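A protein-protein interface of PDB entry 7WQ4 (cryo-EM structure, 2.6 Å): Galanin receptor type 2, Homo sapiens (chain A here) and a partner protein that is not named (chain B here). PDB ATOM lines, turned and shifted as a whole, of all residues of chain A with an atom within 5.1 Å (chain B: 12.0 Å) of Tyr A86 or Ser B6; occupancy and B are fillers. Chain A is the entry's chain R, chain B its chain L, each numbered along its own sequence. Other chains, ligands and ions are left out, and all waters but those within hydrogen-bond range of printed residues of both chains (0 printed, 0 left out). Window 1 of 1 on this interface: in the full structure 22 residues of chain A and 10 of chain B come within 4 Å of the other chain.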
ATOM      1  N   GLN A  82     -12.389   9.194 -10.522  1.00  0.00           N
ATOM      2  CA  GLN A  82     -13.734   8.684 -10.908  1.00  0.00           C
ATOM      3  C   GLN A  82     -14.625   8.617  -9.664  1.00  0.00           C
ATOM      4  O   GLN A  82     -15.831   8.845  -9.806  1.00  0.00           O
ATOM      5  CB  GLN A  82     -13.635   7.365 -11.671  1.00  0.00           C
ATOM      6  CG  GLN A  82     -13.007   7.527 -13.048  1.00  0.00           C
ATOM      7  CD  GLN A  82     -13.653   6.641 -14.082  1.00  0.00           C
ATOM      8  OE1 GLN A  82     -14.391   5.715 -13.759  1.00  0.00           O
ATOM      9  NE2 GLN A  82     -13.374   6.920 -15.345  1.00  0.00           N
ATOM     10  N   ALA A  83     -14.052   8.333  -8.491  1.00  0.00           N
ATOM     11  CA  ALA A  83     -14.837   8.350  -7.261  1.00  0.00           C
ATOM     12  C   ALA A  83     -15.355   9.750  -6.961  1.00  0.00           C
ATOM     13  O   ALA A  83     -16.517   9.921  -6.578  1.00  0.00           O
ATOM     14  CB  ALA A  83     -13.999   7.825  -6.095  1.00  0.00           C
ATOM     15  N   THR A  84     -14.506  10.764  -7.136  1.00  0.00           N
ATOM     16  CA  THR A  84     -14.947  12.141  -6.940  1.00  0.00           C
ATOM     17  C   THR A  84     -15.992  12.535  -7.977  1.00  0.00           C
ATOM     18  O   THR A  84     -16.933  13.277  -7.673  1.00  0.00           O
ATOM     19  CB  THR A  84     -13.747  13.088  -6.995  1.00  0.00           C
ATOM     20  OG1 THR A  84     -12.757  12.661  -6.052  1.00  0.00           O
ATOM     21  CG2 THR A  84     -14.169  14.512  -6.663  1.00  0.00           C
ATOM     22  N   ILE A  85     -15.842  12.045  -9.210  1.00  0.00           N
ATOM     23  CA  ILE A  85     -16.822  12.338 -10.254  1.00  0.00           C
ATOM     24  C   ILE A  85     -18.183  11.755  -9.893  1.00  0.00           C
ATOM     25  O   ILE A  85     -19.208  12.445  -9.961  1.00  0.00           O
ATOM     26  CB  ILE A  85     -16.326  11.816 -11.617  1.00  0.00           C
ATOM     27  CG1 ILE A  85     -15.149  12.657 -12.117  1.00  0.00           C
ATOM     28  CG2 ILE A  85     -17.458  11.817 -12.635  1.00  0.00           C
ATOM     29  CD1 ILE A  85     -14.588  12.191 -13.442  1.00  0.00           C
ATOM     30  N   TYR A  86     -18.216  10.483  -9.499  1.00  0.00           N
ATOM     31  CA  TYR A  86     -19.463   9.820  -9.141  1.00  0.00           C
ATOM     32  C   TYR A  86     -19.980  10.209  -7.762  1.00  0.00           C
ATOM     33  O   TYR A  86     -21.107   9.837  -7.416  1.00  0.00           O
ATOM     34  CB  TYR A  86     -19.293   8.298  -9.211  1.00  0.00           C
ATOM     35  CG  TYR A  86     -19.374   7.738 -10.612  1.00  0.00           C
ATOM     36  CD1 TYR A  86     -18.240   7.627 -11.406  1.00  0.00           C
ATOM     37  CD2 TYR A  86     -20.588   7.323 -11.144  1.00  0.00           C
ATOM     38  CE1 TYR A  86     -18.313   7.117 -12.689  1.00  0.00           C
ATOM     39  CE2 TYR A  86     -20.671   6.810 -12.425  1.00  0.00           C
ATOM     40  CZ  TYR A  86     -19.530   6.710 -13.193  1.00  0.00           C
ATOM     41  OH  TYR A  86     -19.608   6.201 -14.469  1.00  0.00           O
ATOM     42  N   THR A  87     -19.196  10.942  -6.972  1.00  0.00           N
ATOM     43  CA  THR A  87     -19.628  11.401  -5.656  1.00  0.00           C
ATOM     44  C   THR A  87     -20.122  12.844  -5.697  1.00  0.00           C
ATOM     45  O   THR A  87     -21.241  13.135  -5.265  1.00  0.00           O
ATOM     46  CB  THR A  87     -18.485  11.258  -4.642  1.00  0.00           C
ATOM     47  OG1 THR A  87     -18.092   9.884  -4.553  1.00  0.00           O
ATOM     48  CG2 THR A  87     -18.926  11.745  -3.270  1.00  0.00           C
ATOM     49  N   LEU A  88     -19.303  13.754  -6.213  1.00  0.00           N
ATOM     50  CA  LEU A  88     -19.682  15.153  -6.331  1.00  0.00           C
ATOM     51  C   LEU A  88     -20.461  15.387  -7.624  1.00  0.00           C
ATOM     52  O   LEU A  88     -20.547  14.523  -8.498  1.00  0.00           O
ATOM     53  CB  LEU A  88     -18.445  16.049  -6.281  1.00  0.00           C
ATOM     54  CG  LEU A  88     -17.627  15.996  -4.988  1.00  0.00           C
ATOM     55  CD1 LEU A  88     -16.461  16.971  -5.046  1.00  0.00           C
ATOM     56  CD2 LEU A  88     -18.511  16.280  -3.783  1.00  0.00           C
ATOM     57  N   TYR A 271     -27.546   2.572 -13.388  1.00  0.00           N
ATOM     58  CA  TYR A 271     -26.490   3.156 -12.568  1.00  0.00           C
ATOM     59  C   TYR A 271     -25.828   2.101 -11.692  1.00  0.00           C
ATOM     60  O   TYR A 271     -24.601   2.098 -11.526  1.00  0.00           O
ATOM     61  CB  TYR A 271     -27.058   4.290 -11.713  1.00  0.00           C
ATOM     62  CG  TYR A 271     -26.055   4.916 -10.770  1.00  0.00           C
ATOM     63  CD1 TYR A 271     -25.141   5.859 -11.223  1.00  0.00           C
ATOM     64  CD2 TYR A 271     -26.028   4.572  -9.425  1.00  0.00           C
ATOM     65  CE1 TYR A 271     -24.224   6.436 -10.364  1.00  0.00           C
ATOM     66  CE2 TYR A 271     -25.115   5.144  -8.558  1.00  0.00           C
ATOM     67  CZ  TYR A 271     -24.216   6.075  -9.033  1.00  0.00           C
ATOM     68  OH  TYR A 271     -23.304   6.647  -8.176  1.00  0.00           O
ATOM     69  N   ARG A 274     -23.547   0.091 -13.881  1.00  0.00           N
ATOM     70  CA  ARG A 274     -22.333   0.841 -14.193  1.00  0.00           C
ATOM     71  C   ARG A 274     -21.371   0.840 -13.010  1.00  0.00           C
ATOM     72  O   ARG A 274     -20.155   0.675 -13.178  1.00  0.00           O
ATOM     73  CB  ARG A 274     -22.693   2.271 -14.598  1.00  0.00           C
ATOM     74  CG  ARG A 274     -21.499   3.138 -14.966  1.00  0.00           C
ATOM     75  CD  ARG A 274     -20.777   2.599 -16.190  1.00  0.00           C
ATOM     76  NE  ARG A 274     -19.693   3.479 -16.616  1.00  0.00           N
ATOM     77  CZ  ARG A 274     -18.907   3.245 -17.662  1.00  0.00           C
ATOM     78  NH1 ARG A 274     -19.082   2.154 -18.394  1.00  0.00           N
ATOM     79  NH2 ARG A 274     -17.944   4.101 -17.976  1.00  0.00           N
ATOM     80  N   ILE A 275     -21.903   1.026 -11.798  1.00  0.00           N
ATOM     81  CA  ILE A 275     -21.063   0.998 -10.605  1.00  0.00           C
ATOM     82  C   ILE A 275     -20.433  -0.379 -10.428  1.00  0.00           C
ATOM     83  O   ILE A 275     -19.244  -0.498 -10.106  1.00  0.00           O
ATOM     84  CB  ILE A 275     -21.876   1.415  -9.365  1.00  0.00           C
ATOM     85  CG1 ILE A 275     -22.281   2.888  -9.464  1.00  0.00           C
ATOM     86  CG2 ILE A 275     -21.085   1.161  -8.090  1.00  0.00           C
ATOM     87  CD1 ILE A 275     -21.108   3.840  -9.538  1.00  0.00           C
ATOM     88  N   HIS A 278     -17.606  -0.773 -12.948  1.00  0.00           N
ATOM     89  CA  HIS A 278     -16.408  -0.068 -12.500  1.00  0.00           C
ATOM     90  C   HIS A 278     -15.719  -0.816 -11.365  1.00  0.00           C
ATOM     91  O   HIS A 278     -14.485  -0.902 -11.324  1.00  0.00           O
ATOM     92  CB  HIS A 278     -16.761   1.356 -12.071  1.00  0.00           C
ATOM     93  CG  HIS A 278     -16.884   2.317 -13.212  1.00  0.00           C
ATOM     94  ND1 HIS A 278     -17.181   3.650 -13.033  1.00  0.00           N
ATOM     95  CD2 HIS A 278     -16.744   2.138 -14.546  1.00  0.00           C
ATOM     96  CE1 HIS A 278     -17.222   4.252 -14.209  1.00  0.00           C
ATOM     97  NE2 HIS A 278     -16.961   3.356 -15.144  1.00  0.00           N
ATOM     98  N   GLY B   1     -29.795   6.497  -9.266  1.00  0.00           N
ATOM     99  CA  GLY B   1     -29.735   7.935  -9.077  1.00  0.00           C
ATOM    100  C   GLY B   1     -28.731   8.617  -9.986  1.00  0.00           C
ATOM    101  O   GLY B   1     -27.600   8.888  -9.585  1.00  0.00           O
ATOM    102  N   TRP B   2     -29.150   8.894 -11.218  1.00  0.00           N
ATOM    103  CA  TRP B   2     -28.271   9.544 -12.177  1.00  0.00           C
ATOM    104  C   TRP B   2     -28.155  11.036 -11.884  1.00  0.00           C
ATOM    105  O   TRP B   2     -29.104  11.682 -11.432  1.00  0.00           O
ATOM    106  CB  TRP B   2     -28.782   9.331 -13.602  1.00  0.00           C
ATOM    107  CG  TRP B   2     -28.619   7.925 -14.091  1.00  0.00           C
ATOM    108  CD1 TRP B   2     -29.549   6.928 -14.043  1.00  0.00           C
ATOM    109  CD2 TRP B   2     -27.453   7.360 -14.701  1.00  0.00           C
ATOM    110  NE1 TRP B   2     -29.034   5.776 -14.588  1.00  0.00           N
ATOM    111  CE2 TRP B   2     -27.749   6.015 -14.999  1.00  0.00           C
ATOM    112  CE3 TRP B   2     -26.189   7.860 -15.027  1.00  0.00           C
ATOM    113  CZ2 TRP B   2     -26.827   5.164 -15.606  1.00  0.00           C
ATOM    114  CZ3 TRP B   2     -25.275   7.014 -15.628  1.00  0.00           C
ATOM    115  CH2 TRP B   2     -25.598   5.682 -15.911  1.00  0.00           C
ATOM    116  N   THR B   3     -26.970  11.579 -12.148  1.00  0.00           N
ATOM    117  CA  THR B   3     -26.685  12.989 -11.941  1.00  0.00           C
ATOM    118  C   THR B   3     -26.180  13.591 -13.245  1.00  0.00           C
ATOM    119  O   THR B   3     -25.743  12.879 -14.153  1.00  0.00           O
ATOM    120  CB  THR B   3     -25.652  13.198 -10.821  1.00  0.00           C
ATOM    121  OG1 THR B   3     -25.829  12.195  -9.814  1.00  0.00           O
ATOM    122  CG2 THR B   3     -25.819  14.570 -10.181  1.00  0.00           C
ATOM    123  N   LEU B   4     -26.249  14.922 -13.330  1.00  0.00           N
ATOM    124  CA  LEU B   4     -25.786  15.612 -14.531  1.00  0.00           C
ATOM    125  C   LEU B   4     -24.285  15.445 -14.734  1.00  0.00           C
ATOM    126  O   LEU B   4     -23.793  15.581 -15.860  1.00  0.00           O
ATOM    127  CB  LEU B   4     -26.150  17.094 -14.457  1.00  0.00           C
ATOM    128  CG  LEU B   4     -27.642  17.420 -14.374  1.00  0.00           C
ATOM    129  CD1 LEU B   4     -27.862  18.924 -14.313  1.00  0.00           C
ATOM    130  CD2 LEU B   4     -28.391  16.811 -15.550  1.00  0.00           C
ATOM    131  N   ASN B   5     -23.545  15.149 -13.667  1.00  0.00           N
ATOM    132  CA  ASN B   5     -22.107  14.935 -13.758  1.00  0.00           C
ATOM    133  C   ASN B   5     -21.745  13.512 -14.162  1.00  0.00           C
ATOM    134  O   ASN B   5     -20.615  13.279 -14.603  1.00  0.00           O
ATOM    135  CB  ASN B   5     -21.440  15.273 -12.420  1.00  0.00           C
ATOM    136  CG  ASN B   5     -19.929  15.354 -12.524  1.00  0.00           C
ATOM    137  OD1 ASN B   5     -19.382  15.637 -13.590  1.00  0.00           O
ATOM    138  ND2 ASN B   5     -19.244  15.104 -11.414  1.00  0.00           N
ATOM    139  N   SER B   6     -22.670  12.562 -14.032  1.00  0.00           N
ATOM    140  CA  SER B   6     -22.426  11.170 -14.393  1.00  0.00           C
ATOM    141  C   SER B   6     -23.036  10.802 -15.740  1.00  0.00           C
ATOM    142  O   SER B   6     -22.363  10.196 -16.581  1.00  0.00           O
ATOM    143  CB  SER B   6     -22.972  10.240 -13.303  1.00  0.00           C
ATOM    144  OG  SER B   6     -22.342  10.491 -12.058  1.00  0.00           O
ATOM    145  N   ALA B   7     -24.304  11.155 -15.962  1.00  0.00           N
ATOM    146  CA  ALA B   7     -24.935  10.871 -17.246  1.00  0.00           C
ATOM    147  C   ALA B   7     -24.248  11.616 -18.382  1.00  0.00           C
ATOM    148  O   ALA B   7     -24.067  11.057 -19.471  1.00  0.00           O
ATOM    149  CB  ALA B   7     -26.420  11.230 -17.194  1.00  0.00           C
ATOM    150  N   GLY B   8     -23.854  12.866 -18.152  1.00  0.00           N
ATOM    151  CA  GLY B   8     -23.142  13.631 -19.156  1.00  0.00           C
ATOM    152  C   GLY B   8     -21.743  13.108 -19.399  1.00  0.00           C
ATOM    153  O   GLY B   8     -21.239  13.157 -20.525  1.00  0.00           O
ATOM    154  N   TYR B   9     -21.117  12.565 -18.349  1.00  0.00           N
ATOM    155  CA  TYR B   9     -19.747  11.998 -18.472  1.00  0.00           C
ATOM    156  C   TYR B   9     -19.813  10.691 -19.257  1.00  0.00           C
ATOM    157  O   TYR B   9     -18.880  10.395 -20.025  1.00  0.00           O
ATOM    158  CB  TYR B   9     -19.177  11.722 -17.079  1.00  0.00           C
ATOM    159  CG  TYR B   9     -17.808  11.092 -17.039  1.00  0.00           C
ATOM    160  CD1 TYR B   9     -16.711  11.732 -17.591  1.00  0.00           C
ATOM    161  CD2 TYR B   9     -17.607   9.861 -16.439  1.00  0.00           C
ATOM    162  CE1 TYR B   9     -15.451  11.162 -17.553  1.00  0.00           C
ATOM    163  CE2 TYR B   9     -16.354   9.275 -16.393  1.00  0.00           C
ATOM    164  CZ  TYR B   9     -15.271   9.929 -16.954  1.00  0.00           C
ATOM    165  OH  TYR B   9     -14.031   9.361 -16.915  1.00  0.00           O
ATOM    166  N   LEU B  10     -20.895   9.939 -19.076  1.00  0.00           N
ATOM    167  CA  LEU B  10     -21.003   8.636 -19.722  1.00  0.00           C
ATOM    168  C   LEU B  10     -21.508   8.733 -21.158  1.00  0.00           C
ATOM    169  O   LEU B  10     -20.976   8.055 -22.044  1.00  0.00           O
ATOM    170  CB  LEU B  10     -21.923   7.721 -18.909  1.00  0.00           C
ATOM    171  CG  LEU B  10     -22.124   6.303 -19.449  1.00  0.00           C
ATOM    172  CD1 LEU B  10     -20.790   5.590 -19.602  1.00  0.00           C
ATOM    173  CD2 LEU B  10     -23.053   5.515 -18.541  1.00  0.00           C
ATOM    174  N   LEU B  11     -22.520   9.562 -21.411  1.00  0.00           N
ATOM    175  CA  LEU B  11     -23.120   9.670 -22.733  1.00  0.00           C
ATOM    176  C   LEU B  11     -22.556  10.814 -23.563  1.00  0.00           C
ATOM    177  O   LEU B  11     -22.865  10.901 -24.756  1.00  0.00           O
ATOM    178  CB  LEU B  11     -24.641   9.836 -22.613  1.00  0.00           C
ATOM    179  CG  LEU B  11     -25.398   8.702 -21.921  1.00  0.00           C
ATOM    180  CD1 LEU B  11     -26.882   9.020 -21.843  1.00  0.00           C
ATOM    181  CD2 LEU B  11     -25.167   7.384 -22.642  1.00  0.00           C
ATOM    182  N   GLY B  12     -21.745  11.687 -22.972  1.00  0.00           N
ATOM    183  CA  GLY B  12     -21.180  12.804 -23.690  1.00  0.00           C
ATOM    184  C   GLY B  12     -22.050  14.042 -23.601  1.00  0.00           C
ATOM    185  O   GLY B  12     -22.862  14.194 -22.683  1.00  0.00           O
ATOM    186  N   PRO B  13     -21.891  14.963 -24.563  1.00  0.00           N
ATOM    187  CA  PRO B  13     -22.669  16.207 -24.621  1.00  0.00           C
ATOM    188  C   PRO B  13     -24.170  15.960 -24.747  1.00  0.00           C
ATOM    189  O   PRO B  13     -24.952  16.825 -24.354  1.00  0.00           O
ATOM    190  CB  PRO B  13     -22.128  16.902 -25.875  1.00  0.00           C
ATOM    191  CG  PRO B  13     -20.771  16.322 -26.077  1.00  0.00           C
ATOM    192  CD  PRO B  13     -20.883  14.897 -25.634  1.00  0.00           C
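OH of Tyr B9 lies within hydrogen-bond range of NE2 of Gln A82, at 3.0 Å. O of Ile A85 is in hydrogen-bond range of ND2 of Asn B5 (3.0 Å). The backbone carbonyl oxygen of Leu A88 lies within hydrogen-bond range of the side-chain amide nitrogen of Asn B5 (3.2 Å).
NE of Arg A274 lies within hydrogen-bond range of OH of Tyr A86 (3.5 Å). NH2 of Arg A274 lies within hydrogen-bond range of NE2 of His A278, 3.1 Å away.
Among the printed residues, merely in contact across the chains: Tyr A271 with Trp B2 (3.5 Å), Arg A274 with Leu B10 (3.6 Å) and Tyr A86 with Ser B6 (3.7 Å).
Gln A82 touches just one residue of chain B: Tyr B9. No residue of chain B comes within 4 Å of Ala A83. No residue of chain B comes within 4 Å of Thr A84. Tyr A86 touches just one residue of chain B: Ser B6. No residue of chain B comes within 4 Å of Thr A87. Printed residues of chain B within 4 Å of Tyr A271: Trp B2 (3.5 Å). Arg A274 touches just one residue of chain B: Leu B10 (3.6 Å). No residue of chain B comes within 4 Å of Ile A275. Of the printed residues of chain A, Asn B5 touches Ile A85 (3.0 Å) and Leu A88 (3.2 Å). Ser B6 touches one residue of chain A. The nearest residue of chain A that does not touch Ser B6 is Ile A85 (4.2 Å).
Of the 13 printed residues of chain B, 5 touch a printed residue of chain A. Hydrophobic or aromatic side chains of chain B that line the printed part of chain A: Trp B2, Tyr B9 and Leu B10. Of the 11 printed residues of chain A, 6 touch a printed residue of chain B. Hydrophobic or aromatic side chains of chain A within 4 Å of the printed part of chain B: Ile A85, Tyr A86 and Tyr A271. Among the printed residues, no Asp or Glu carboxylate lies within 4 Å of a Lys or Arg side-chain nitrogen of the other chain.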
